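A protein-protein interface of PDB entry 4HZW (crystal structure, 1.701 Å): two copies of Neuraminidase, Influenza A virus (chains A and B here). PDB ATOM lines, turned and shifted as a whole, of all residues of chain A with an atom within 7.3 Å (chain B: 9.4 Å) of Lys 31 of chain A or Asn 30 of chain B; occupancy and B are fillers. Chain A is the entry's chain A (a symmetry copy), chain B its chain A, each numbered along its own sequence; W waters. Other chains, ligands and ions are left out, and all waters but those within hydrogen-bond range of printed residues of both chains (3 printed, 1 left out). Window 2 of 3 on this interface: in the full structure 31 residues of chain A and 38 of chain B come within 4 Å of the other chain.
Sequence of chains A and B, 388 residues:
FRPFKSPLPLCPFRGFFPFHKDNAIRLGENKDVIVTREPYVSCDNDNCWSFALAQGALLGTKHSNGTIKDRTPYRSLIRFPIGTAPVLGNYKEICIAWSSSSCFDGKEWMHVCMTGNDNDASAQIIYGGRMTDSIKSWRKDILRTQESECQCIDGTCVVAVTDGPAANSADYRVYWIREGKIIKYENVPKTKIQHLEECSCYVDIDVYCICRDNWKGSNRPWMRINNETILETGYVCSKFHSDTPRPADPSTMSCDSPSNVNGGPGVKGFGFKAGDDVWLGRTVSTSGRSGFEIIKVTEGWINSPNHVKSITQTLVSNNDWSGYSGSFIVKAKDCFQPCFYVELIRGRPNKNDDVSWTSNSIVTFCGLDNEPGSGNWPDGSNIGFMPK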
ATOM      1  N   LEU A  27      23.716  11.265  25.624  1.00  0.00           N
ATOM      2  CA  LEU A  27      23.165  11.065  26.965  1.00  0.00           C
ATOM      3  C   LEU A  27      21.696  11.468  27.054  1.00  0.00           C
ATOM      4  O   LEU A  27      21.040  11.220  28.069  1.00  0.00           O
ATOM      5  CB  LEU A  27      23.982  11.859  27.987  1.00  0.00           C
ATOM      6  CG  LEU A  27      25.408  11.351  28.193  1.00  0.00           C
ATOM      7  CD1 LEU A  27      26.246  12.364  28.978  1.00  0.00           C
ATOM      8  CD2 LEU A  27      25.373  10.011  28.915  1.00  0.00           C
ATOM      9  N   GLY A  28      21.183  12.092  25.998  1.00  0.00           N
ATOM     10  CA  GLY A  28      19.806  12.548  25.980  1.00  0.00           C
ATOM     11  C   GLY A  28      18.864  11.556  25.325  1.00  0.00           C
ATOM     12  O   GLY A  28      17.682  11.845  25.122  1.00  0.00           O
ATOM     13  N   GLU A  29      19.381  10.376  25.011  1.00  0.00           N
ATOM     14  CA  GLU A  29      18.594   9.359  24.328  1.00  0.00           C
ATOM     15  C   GLU A  29      17.316   8.978  25.082  1.00  0.00           C
ATOM     16  O   GLU A  29      16.325   8.588  24.463  1.00  0.00           O
ATOM     17  CB  GLU A  29      19.443   8.113  24.055  1.00  0.00           C
ATOM     18  CG  GLU A  29      18.757   7.109  23.140  1.00  0.00           C
ATOM     19  CD  GLU A  29      19.439   5.758  23.160  1.00  0.00           C
ATOM     20  OE1 GLU A  29      20.685   5.735  23.194  1.00  0.00           O
ATOM     21  OE2 GLU A  29      18.726   4.728  23.160  1.00  0.00           O
ATOM     22  N   ASN A  30      17.331   9.100  26.409  1.00  0.00           N
ATOM     23  CA  ASN A  30      16.169   8.724  27.223  1.00  0.00           C
ATOM     24  C   ASN A  30      15.376   9.941  27.711  1.00  0.00           C
ATOM     25  O   ASN A  30      14.662   9.864  28.713  1.00  0.00           O
ATOM     26  CB  ASN A  30      16.597   7.845  28.410  1.00  0.00           C
ATOM     27  CG  ASN A  30      15.465   6.972  28.945  1.00  0.00           C
ATOM     28  OD1 ASN A  30      15.303   6.821  30.159  1.00  0.00           O
ATOM     29  ND2 ASN A  30      14.685   6.387  28.039  1.00  0.00           N
ATOM     30  N   LYS A  31      15.518  11.053  26.994  1.00  0.00           N
ATOM     31  CA  LYS A  31      14.719  12.268  27.220  1.00  0.00           C
ATOM     32  C   LYS A  31      15.019  13.010  28.532  1.00  0.00           C
ATOM     33  O   LYS A  31      14.145  13.680  29.087  1.00  0.00           O
ATOM     34  CB  LYS A  31      13.220  11.955  27.115  1.00  0.00           C
ATOM     35  CG  LYS A  31      12.845  11.172  25.858  1.00  0.00           C
ATOM     36  CD  LYS A  31      11.337  11.046  25.689  1.00  0.00           C
ATOM     37  CE  LYS A  31      10.991  10.248  24.443  1.00  0.00           C
ATOM     38  NZ  LYS A  31       9.510  10.122  24.257  1.00  0.00           N
ATOM     39  N   ASP A  32      16.251  12.906  29.021  1.00  0.00           N
ATOM     40  CA  ASP A  32      16.628  13.588  30.261  1.00  0.00           C
ATOM     41  C   ASP A  32      17.189  14.983  30.014  1.00  0.00           C
ATOM     42  O   ASP A  32      17.207  15.829  30.917  1.00  0.00           O
ATOM     43  CB  ASP A  32      17.673  12.772  31.023  1.00  0.00           C
ATOM     44  CG  ASP A  32      17.128  11.454  31.533  1.00  0.00           C
ATOM     45  OD1 ASP A  32      16.347  11.478  32.506  1.00  0.00           O
ATOM     46  OD2 ASP A  32      17.476  10.395  30.963  1.00  0.00           O
ATOM     47  N   VAL A  33      17.651  15.218  28.791  1.00  0.00           N
ATOM     48  CA  VAL A  33      18.471  16.385  28.500  1.00  0.00           C
ATOM     49  C   VAL A  33      17.654  17.551  27.953  1.00  0.00           C
ATOM     50  O   VAL A  33      16.774  17.374  27.113  1.00  0.00           O
ATOM     51  CB  VAL A  33      19.637  16.009  27.548  1.00  0.00           C
ATOM     52  CG1 VAL A  33      20.455  17.234  27.178  1.00  0.00           C
ATOM     53  CG2 VAL A  33      20.524  14.961  28.223  1.00  0.00           C
ATOM     54  N   ILE A  34      17.948  18.742  28.455  1.00  0.00           N
ATOM     55  CA  ILE A  34      17.289  19.962  28.004  1.00  0.00           C
ATOM     56  C   ILE A  34      17.741  20.334  26.590  1.00  0.00           C
ATOM     57  O   ILE A  34      18.928  20.280  26.276  1.00  0.00           O
ATOM     58  CB  ILE A  34      17.594  21.132  28.979  1.00  0.00           C
ATOM     59  CG1 ILE A  34      17.127  20.780  30.394  1.00  0.00           C
ATOM     60  CG2 ILE A  34      16.944  22.435  28.496  1.00  0.00           C
ATOM     61  CD1 ILE A  34      17.664  21.717  31.473  1.00  0.00           C
ATOM     62  N   LEU A  58      12.450  19.308  26.901  1.00  0.00           N
ATOM     63  CA  LEU A  58      13.386  18.186  26.977  1.00  0.00           C
ATOM     64  C   LEU A  58      13.538  17.513  25.616  1.00  0.00           C
ATOM     65  O   LEU A  58      12.570  17.380  24.868  1.00  0.00           O
ATOM     66  CB  LEU A  58      12.909  17.164  28.010  1.00  0.00           C
ATOM     67  CG  LEU A  58      12.887  17.656  29.460  1.00  0.00           C
ATOM     68  CD1 LEU A  58      12.401  16.539  30.372  1.00  0.00           C
ATOM     69  CD2 LEU A  58      14.255  18.145  29.893  1.00  0.00           C
ATOM     70  N   LEU A  59      14.755  17.072  25.315  1.00  0.00           N
ATOM     71  CA  LEU A  59      15.087  16.479  24.025  1.00  0.00           C
ATOM     72  C   LEU A  59      14.275  15.207  23.759  1.00  0.00           C
ATOM     73  O   LEU A  59      14.239  14.289  24.585  1.00  0.00           O
ATOM     74  CB  LEU A  59      16.593  16.192  23.980  1.00  0.00           C
ATOM     75  CG  LEU A  59      17.309  15.819  22.673  1.00  0.00           C
ATOM     76  CD1 LEU A  59      16.893  14.437  22.188  1.00  0.00           C
ATOM     77  CD2 LEU A  59      17.073  16.862  21.615  1.00  0.00           C
ATOM     78  N   GLY A  60      13.596  15.171  22.618  1.00  0.00           N
ATOM     79  CA  GLY A  60      12.830  14.000  22.233  1.00  0.00           C
ATOM     80  C   GLY A  60      11.401  13.989  22.732  1.00  0.00           C
ATOM     81  O   GLY A  60      10.666  13.032  22.487  1.00  0.00           O
ATOM     82  N   THR A  61      11.000  15.038  23.448  1.00  0.00           N
ATOM     83  CA  THR A  61       9.607  15.177  23.843  1.00  0.00           C
ATOM     84  C   THR A  61       8.847  15.910  22.742  1.00  0.00           C
ATOM     85  O   THR A  61       9.448  16.444  21.805  1.00  0.00           O
ATOM     86  CB  THR A  61       9.447  15.925  25.187  1.00  0.00           C
ATOM     87  OG1 THR A  61       9.930  17.270  25.046  1.00  0.00           O
ATOM     88  CG2 THR A  61      10.217  15.212  26.292  1.00  0.00           C
ATOM     89  N   LYS A  62       7.524  15.918  22.831  1.00  0.00           N
ATOM     90  CA  LYS A  62       6.738  16.583  21.798  1.00  0.00           C
ATOM     91  C   LYS A  62       7.021  18.086  21.739  1.00  0.00           C
ATOM     92  O   LYS A  62       6.994  18.685  20.664  1.00  0.00           O
ATOM     93  CB  LYS A  62       5.246  16.295  21.982  1.00  0.00           C
ATOM     94  CG  LYS A  62       4.901  14.832  21.754  1.00  0.00           C
ATOM     95  CD  LYS A  62       3.424  14.536  21.954  1.00  0.00           C
ATOM     96  CE  LYS A  62       3.139  13.066  21.687  1.00  0.00           C
ATOM     97  NZ  LYS A  62       1.698  12.726  21.840  1.00  0.00           N
ATOM     98  N   VAL A  87      20.565  18.909  32.527  1.00  0.00           N
ATOM     99  CA  VAL A  87      19.362  18.195  32.942  1.00  0.00           C
ATOM    100  C   VAL A  87      18.646  18.980  34.037  1.00  0.00           C
ATOM    101  O   VAL A  87      19.209  19.916  34.620  1.00  0.00           O
ATOM    102  CB  VAL A  87      19.683  16.751  33.415  1.00  0.00           C
ATOM    103  CG1 VAL A  87      20.412  15.991  32.316  1.00  0.00           C
ATOM    104  CG2 VAL A  87      20.528  16.769  34.678  1.00  0.00           C
ATOM    105  N   LEU A  88      17.399  18.618  34.303  1.00  0.00           N
ATOM    106  CA  LEU A  88      16.602  19.372  35.256  1.00  0.00           C
ATOM    107  C   LEU A  88      17.232  19.335  36.643  1.00  0.00           C
ATOM    108  O   LEU A  88      17.080  20.270  37.428  1.00  0.00           O
ATOM    109  CB  LEU A  88      15.167  18.845  35.290  1.00  0.00           C
ATOM    110  CG  LEU A  88      14.369  19.099  34.009  1.00  0.00           C
ATOM    111  CD1 LEU A  88      12.998  18.461  34.108  1.00  0.00           C
ATOM    112  CD2 LEU A  88      14.244  20.592  33.748  1.00  0.00           C
ATOM    113  N   MET A 386      17.857   7.982  18.367  1.00  0.00           N
ATOM    114  CA  MET A 386      17.208   9.035  19.141  1.00  0.00           C
ATOM    115  C   MET A 386      15.694   9.092  18.980  1.00  0.00           C
ATOM    116  O   MET A 386      15.158   8.809  17.902  1.00  0.00           O
ATOM    117  CB  MET A 386      17.804  10.403  18.773  1.00  0.00           C
ATOM    118  CG  MET A 386      19.313  10.494  18.954  1.00  0.00           C
ATOM    119  SD  MET A 386      19.848  10.317  20.673  1.00  0.00           S
ATOM    120  CE  MET A 386      19.148  11.812  21.410  1.00  0.00           C
ATOM    121  N   PRO A 387      14.995   9.471  20.059  1.00  0.00           N
ATOM    122  CA  PRO A 387      13.578   9.800  19.929  1.00  0.00           C
ATOM    123  C   PRO A 387      13.476  11.004  19.003  1.00  0.00           C
ATOM    124  O   PRO A 387      14.301  11.908  19.109  1.00  0.00           O
ATOM    125  CB  PRO A 387      13.168  10.181  21.356  1.00  0.00           C
ATOM    126  CG  PRO A 387      14.453  10.557  22.042  1.00  0.00           C
ATOM    127  CD  PRO A 387      15.512   9.706  21.417  1.00  0.00           C
ATOM    128  N   LYS A 388      12.494  11.011  18.108  1.00  0.00           N
ATOM    129  CA  LYS A 388      12.409  12.040  17.078  1.00  0.00           C
ATOM    130  C   LYS A 388      11.650  13.281  17.534  1.00  0.00           C
ATOM    131  O   LYS A 388      10.981  13.292  18.570  1.00  0.00           O
ATOM    132  CB  LYS A 388      11.774  11.465  15.810  1.00  0.00           C
ATOM    133  CG  LYS A 388      12.561  10.303  15.209  1.00  0.00           C
ATOM    134  CD  LYS A 388      11.893   9.768  13.953  1.00  0.00           C
ATOM    135  CE  LYS A 388      12.679   8.606  13.361  1.00  0.00           C
ATOM    136  NZ  LYS A 388      14.078   8.994  13.019  1.00  0.00           N
ATOM    137  OXT LYS A 388      11.695  14.309  16.865  1.00  0.00           O
ATOM    138  N   ALA B  24       7.890  25.317  33.474  1.00  0.00           N
ATOM    139  CA  ALA B  24       7.796  24.057  34.216  1.00  0.00           C
ATOM    140  C   ALA B  24       6.833  23.048  33.612  1.00  0.00           C
ATOM    141  O   ALA B  24       7.090  21.846  33.668  1.00  0.00           O
ATOM    142  CB  ALA B  24       7.432  24.309  35.681  1.00  0.00           C
ATOM    143  N   ILE B  25       5.718  23.513  33.057  1.00  0.00           N
ATOM    144  CA  ILE B  25       4.755  22.566  32.496  1.00  0.00           C
ATOM    145  C   ILE B  25       5.349  21.941  31.229  1.00  0.00           C
ATOM    146  O   ILE B  25       5.366  20.720  31.082  1.00  0.00           O
ATOM    147  CB  ILE B  25       3.375  23.196  32.228  1.00  0.00           C
ATOM    148  CG1 ILE B  25       2.796  23.804  33.514  1.00  0.00           C
ATOM    149  CG2 ILE B  25       2.414  22.161  31.640  1.00  0.00           C
ATOM    150  CD1 ILE B  25       2.564  22.807  34.625  1.00  0.00           C
ATOM    151  N   ARG B  26       5.874  22.777  30.341  1.00  0.00           N
ATOM    152  CA  ARG B  26       6.561  22.283  29.145  1.00  0.00           C
ATOM    153  C   ARG B  26       7.608  21.224  29.482  1.00  0.00           C
ATOM    154  O   ARG B  26       7.683  20.173  28.837  1.00  0.00           O
ATOM    155  CB  ARG B  26       7.239  23.439  28.403  1.00  0.00           C
ATOM    156  CG  ARG B  26       6.278  24.391  27.709  1.00  0.00           C
ATOM    157  CD  ARG B  26       6.999  25.629  27.206  1.00  0.00           C
ATOM    158  NE  ARG B  26       8.111  25.311  26.298  1.00  0.00           N
ATOM    159  CZ  ARG B  26       8.010  25.247  24.974  1.00  0.00           C
ATOM    160  NH1 ARG B  26       9.081  24.966  24.234  1.00  0.00           N
ATOM    161  NH2 ARG B  26       6.844  25.467  24.382  1.00  0.00           N
ATOM    162  N   LEU B  27       8.414  21.506  30.498  1.00  0.00           N
ATOM    163  CA  LEU B  27       9.505  20.614  30.892  1.00  0.00           C
ATOM    164  C   LEU B  27       9.009  19.402  31.675  1.00  0.00           C
ATOM    165  O   LEU B  27       9.778  18.476  31.949  1.00  0.00           O
ATOM    166  CB  LEU B  27      10.532  21.384  31.726  1.00  0.00           C
ATOM    167  CG  LEU B  27      11.308  22.449  30.953  1.00  0.00           C
ATOM    168  CD1 LEU B  27      12.074  23.371  31.905  1.00  0.00           C
ATOM    169  CD2 LEU B  27      12.261  21.776  29.976  1.00  0.00           C
ATOM    170  N   GLY B  28       7.731  19.408  32.040  1.00  0.00           N
ATOM    171  CA  GLY B  28       7.155  18.325  32.812  1.00  0.00           C
ATOM    172  C   GLY B  28       6.469  17.284  31.949  1.00  0.00           C
ATOM    173  O   GLY B  28       5.826  16.363  32.459  1.00  0.00           O
ATOM    174  N   GLU B  29       6.620  17.417  30.638  1.00  0.00           N
ATOM    175  CA  GLU B  29       5.964  16.514  29.703  1.00  0.00           C
ATOM    176  C   GLU B  29       6.318  15.042  29.936  1.00  0.00           C
ATOM    177  O   GLU B  29       5.511  14.158  29.644  1.00  0.00           O
ATOM    178  CB  GLU B  29       6.277  16.915  28.257  1.00  0.00           C
ATOM    179  CG  GLU B  29       5.440  16.165  27.232  1.00  0.00           C
ATOM    180  CD  GLU B  29       5.991  16.307  25.830  1.00  0.00           C
ATOM    181  OE1 GLU B  29       6.440  17.420  25.490  1.00  0.00           O
ATOM    182  OE2 GLU B  29       5.989  15.303  25.081  1.00  0.00           O
ATOM    183  N   ASN B  30       7.511  14.778  30.468  1.00  0.00           N
ATOM    184  CA  ASN B  30       7.957  13.399  30.694  1.00  0.00           C
ATOM    185  C   ASN B  30       7.866  12.986  32.167  1.00  0.00           C
ATOM    186  O   ASN B  30       8.565  12.072  32.608  1.00  0.00           O
ATOM    187  CB  ASN B  30       9.386  13.194  30.163  1.00  0.00           C
ATOM    188  CG  ASN B  30       9.699  11.735  29.839  1.00  0.00           C
ATOM    189  OD1 ASN B  30      10.791  11.243  30.134  1.00  0.00           O
ATOM    190  ND2 ASN B  30       8.744  11.044  29.222  1.00  0.00           N
ATOM    191  N   LYS B  31       7.003  13.676  32.911  1.00  0.00           N
ATOM    192  CA  LYS B  31       6.670  13.320  34.300  1.00  0.00           C
ATOM    193  C   LYS B  31       7.803  13.534  35.316  1.00  0.00           C
ATOM    194  O   LYS B  31       7.870  12.842  36.335  1.00  0.00           O
ATOM    195  CB  LYS B  31       6.149  11.879  34.378  1.00  0.00           C
ATOM    196  CG  LYS B  31       5.052  11.569  33.361  1.00  0.00           C
ATOM    197  CD  LYS B  31       4.425  10.200  33.591  1.00  0.00           C
ATOM    198  CE  LYS B  31       3.351   9.909  32.557  1.00  0.00           C
ATOM    199  NZ  LYS B  31       2.719   8.568  32.775  1.00  0.00           N
ATOM    200  N   ASP B  32       8.683  14.496  35.053  1.00  0.00           N
ATOM    201  CA  ASP B  32       9.788  14.775  35.971  1.00  0.00           C
ATOM    202  C   ASP B  32       9.431  15.829  37.013  1.00  0.00           C
ATOM    203  O   ASP B  32      10.073  15.922  38.067  1.00  0.00           O
ATOM    204  CB  ASP B  32      11.017  15.255  35.197  1.00  0.00           C
ATOM    205  CG  ASP B  32      11.603  14.179  34.306  1.00  0.00           C
ATOM    206  OD1 ASP B  32      12.230  13.245  34.846  1.00  0.00           O
ATOM    207  OD2 ASP B  32      11.437  14.263  33.068  1.00  0.00           O
ATOM    208  N   VAL B  33       8.411  16.625  36.712  1.00  0.00           N
ATOM    209  CA  VAL B  33       8.151  17.843  37.463  1.00  0.00           C
ATOM    210  C   VAL B  33       7.114  17.642  38.564  1.00  0.00           C
ATOM    211  O   VAL B  33       6.094  16.985  38.367  1.00  0.00           O
ATOM    212  CB  VAL B  33       7.750  18.999  36.509  1.00  0.00           C
ATOM    213  CG1 VAL B  33       7.404  20.256  37.287  1.00  0.00           C
ATOM    214  CG2 VAL B  33       8.900  19.274  35.537  1.00  0.00           C
ATOM    215  N   ILE B  34       7.402  18.202  39.732  1.00  0.00           N
ATOM    216  CA  ILE B  34       6.493  18.138  40.871  1.00  0.00           C
ATOM    217  C   ILE B  34       5.263  19.019  40.636  1.00  0.00           C
ATOM    218  O   ILE B  34       5.381  20.151  40.172  1.00  0.00           O
ATOM    219  CB  ILE B  34       7.222  18.587  42.166  1.00  0.00           C
ATOM    220  CG1 ILE B  34       8.443  17.700  42.424  1.00  0.00           C
ATOM    221  CG2 ILE B  34       6.270  18.568  43.369  1.00  0.00           C
ATOM    222  CD1 ILE B  34       9.397  18.253  43.480  1.00  0.00           C
ATOM    223  N   LEU B  58       4.030  13.793  41.200  1.00  0.00           N
ATOM    224  CA  LEU B  58       4.664  14.232  39.957  1.00  0.00           C
ATOM    225  C   LEU B  58       3.620  14.463  38.868  1.00  0.00           C
ATOM    226  O   LEU B  58       2.645  13.720  38.763  1.00  0.00           O
ATOM    227  CB  LEU B  58       5.684  13.195  39.484  1.00  0.00           C
ATOM    228  CG  LEU B  58       6.893  12.996  40.403  1.00  0.00           C
ATOM    229  CD1 LEU B  58       7.821  11.948  39.808  1.00  0.00           C
ATOM    230  CD2 LEU B  58       7.632  14.302  40.625  1.00  0.00           C
ATOM    231  N   LEU B  59       3.848  15.485  38.048  1.00  0.00           N
ATOM    232  CA  LEU B  59       2.910  15.890  37.007  1.00  0.00           C
ATOM    233  C   LEU B  59       2.686  14.776  35.981  1.00  0.00           C
ATOM    234  O   LEU B  59       3.640  14.224  35.420  1.00  0.00           O
ATOM    235  CB  LEU B  59       3.433  17.165  36.335  1.00  0.00           C
ATOM    236  CG  LEU B  59       2.558  17.999  35.387  1.00  0.00           C
ATOM    237  CD1 LEU B  59       2.289  17.258  34.084  1.00  0.00           C
ATOM    238  CD2 LEU B  59       1.273  18.404  36.058  1.00  0.00           C
ATOM    239  N   GLY B  60       1.425  14.423  35.761  1.00  0.00           N
ATOM    240  CA  GLY B  60       1.084  13.414  34.775  1.00  0.00           C
ATOM    241  C   GLY B  60       1.071  11.995  35.303  1.00  0.00           C
ATOM    242  O   GLY B  60       0.820  11.056  34.548  1.00  0.00           O
ATOM    243  N   THR B  61       1.356  11.825  36.593  1.00  0.00           N
ATOM    244  CA  THR B  61       1.225  10.516  37.213  1.00  0.00           C
ATOM    245  C   THR B  61      -0.201  10.349  37.728  1.00  0.00           C
ATOM    246  O   THR B  61      -0.982  11.305  37.754  1.00  0.00           O
ATOM    247  CB  THR B  61       2.233  10.309  38.367  1.00  0.00           C
ATOM    248  OG1 THR B  61       1.959  11.248  39.417  1.00  0.00           O
ATOM    249  CG2 THR B  61       3.662  10.491  37.870  1.00  0.00           C
ATOM    250  N   VAL B  87      11.960  19.648  40.498  1.00  0.00           N
ATOM    251  CA  VAL B  87      12.104  18.210  40.299  1.00  0.00           C
ATOM    252  C   VAL B  87      12.691  17.571  41.553  1.00  0.00           C
ATOM    253  O   VAL B  87      13.200  18.266  42.444  1.00  0.00           O
ATOM    254  CB  VAL B  87      12.971  17.885  39.053  1.00  0.00           C
ATOM    255  CG1 VAL B  87      12.378  18.545  37.817  1.00  0.00           C
ATOM    256  CG2 VAL B  87      14.403  18.351  39.251  1.00  0.00           C
ATOM    257  N   PHE B 385      -0.124  17.813  24.318  1.00  0.00           N
ATOM    258  CA  PHE B 385       1.122  17.035  24.372  1.00  0.00           C
ATOM    259  C   PHE B 385       1.329  16.369  25.730  1.00  0.00           C
ATOM    260  O   PHE B 385       2.176  15.485  25.871  1.00  0.00           O
ATOM    261  CB  PHE B 385       2.337  17.935  24.111  1.00  0.00           C
ATOM    262  CG  PHE B 385       2.485  18.397  22.683  1.00  0.00           C
ATOM    263  CD1 PHE B 385       1.684  17.889  21.673  1.00  0.00           C
ATOM    264  CD2 PHE B 385       3.448  19.341  22.358  1.00  0.00           C
ATOM    265  CE1 PHE B 385       1.838  18.328  20.358  1.00  0.00           C
ATOM    266  CE2 PHE B 385       3.610  19.785  21.043  1.00  0.00           C
ATOM    267  CZ  PHE B 385       2.801  19.277  20.047  1.00  0.00           C
ATOM    268  N   MET B 386       0.572  16.805  26.732  1.00  0.00           N
ATOM    269  CA  MET B 386       0.828  16.397  28.110  1.00  0.00           C
ATOM    270  C   MET B 386       0.166  15.084  28.510  1.00  0.00           C
ATOM    271  O   MET B 386      -0.934  14.759  28.049  1.00  0.00           O
ATOM    272  CB  MET B 386       0.377  17.502  29.078  1.00  0.00           C
ATOM    273  CG  MET B 386       1.022  18.857  28.822  1.00  0.00           C
ATOM    274  SD  MET B 386       2.814  18.866  29.070  1.00  0.00           S
ATOM    275  CE  MET B 386       2.919  18.574  30.851  1.00  0.00           C
ATOM    276  N   PRO B 387       0.837  14.323  29.387  1.00  0.00           N
ATOM    277  CA  PRO B 387       0.174  13.185  30.018  1.00  0.00           C
ATOM    278  C   PRO B 387      -0.981  13.735  30.843  1.00  0.00           C
ATOM    279  O   PRO B 387      -0.816  14.771  31.481  1.00  0.00           O
ATOM    280  CB  PRO B 387       1.259  12.602  30.930  1.00  0.00           C
ATOM    281  CG  PRO B 387       2.228  13.732  31.153  1.00  0.00           C
ATOM    282  CD  PRO B 387       2.199  14.545  29.899  1.00  0.00           C
HETATM  283  O   HOH W   1      15.016  13.485  34.166  1.00  0.00           O
HETATM  284  O   HOH W   2       9.616  18.973  27.206  1.00  0.00           O
HETATM  285  O   HOH W   3      12.183   8.743  29.557  1.00  0.00           O
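Lys 31 of chain A touches just one residue of chain B: Asn 30 (3.9 Å). Of the printed residues of chain A, Asn 30 of chain B touches Lys 31. Asn 30 of chain A touches none of the printed residues of chain B. No residue of chain B comes within 4 Å of Asp 32 of chain A. No residue of chain B comes within 4 Å of Gly 60 of chain A. Printed residues of chain B within 4 Å of Leu 88 of chain A: Leu 27, Asp 32 and Val 87. Printed residues of chain B within 4 Å of Lys 62 of chain A: Glu 29 (2.8 Å) and Phe 385 (3.5 Å). Ile 25 of chain B touches none of the printed residues of chain A. Ala 24 of chain B touches none of the printed residues of chain A. The nearest printed residue of chain B that does not touch Leu 88 of chain A is Val 33 of chain B (4.4 Å).
Lys 31 of chain A touches Asn 30 of chain B, but with the chains exchanged Asn 30 of chain A does not touch Lys 31 of chain B (9.5 Å). Leu 58 of chain A touches Leu 27 of chain B, but with the chains exchanged Leu 27 of chain A does not touch Leu 58 of chain B (17.7 Å). Leu 58 of chain A touches Asp 32 of chain B, but with the chains exchanged Asp 32 of chain A does not touch Leu 58 of chain B (11.2 Å). Thr 61 of chain A touches Glu 29 of chain B, but with the chains exchanged Glu 29 of chain A does not touch Thr 61 of chain B (18.5 Å). Positions printed for both chains: 27, 28, 29, 30, 31, 32, 33, 34, 58, 59, 60, 61, 87, 386 and 387. Of the 9 pairs that touch across the chains among the printed residues, none has its exchanged pair printed and touching as well.
Water W2 lies within hydrogen-bond range of the side-chain hydroxyl (OG1) of Thr 61 of chain A (2.8 Å), the backbone carbonyl oxygen (O) of Arg 26 of chain B (2.8 Å) and the backbone NH (N) of Leu 58 of chain A (2.9 Å). Water W3 lies within hydrogen-bond range of the backbone carbonyl oxygen of Asn 30 of chain A and the side-chain amide oxygen of Asn 30 of chain B. Water W1 lies within hydrogen-bond range of the side-chain carboxylate (OD1) of Asp 32 of chain B (2.9 Å) and the side-chain carboxylate (OD1) of Asp 32 of chain A (2.9 Å).
The side-chain carboxylate (OE2) of Glu 29 of chain B lies within hydrogen-bond range of the backbone NH (N) of Lys 62 of chain A, 2.8 Å away.
The side-chain hydroxyl (OG1) of Thr 61 of chain A lies within hydrogen-bond range of the backbone carbonyl oxygen (O) of Leu 58 of chain A, 2.6 Å away.
Among the printed residues, merely in contact across the chains: Lys 31 of chain A with Asn 30 of chain B (3.9 Å), Leu 58 of chain A with Leu 27 of chain B (3.6 Å), Leu 58 of chain A with Asp 32 of chain B (3.7 Å), Thr 61 of chain A with Glu 29 of chain B (3.4 Å), Lys 62 of chain A with Phe 385 of chain B (3.5 Å), Leu 88 of chain A with Leu 27 of chain B (3.9 Å), Leu 88 of chain A with Asp 32 of chain B (3.9 Å) and Leu 88 of chain A with Val 87 of chain B (3.8 Å).
Of the 19 printed residues of chain B, 6 touch a printed residue of chain A. Hydrophobic or aromatic side chains of chain B within 4 Å of the printed part of chain A: Leu 27, Val 87 and Phe 385. Among the printed residues, 9 pairs touch across the chains. Among the printed residues, no Asp or Glu carboxylate lies within 4 Å of a Lys or Arg side-chain nitrogen of the other chain.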
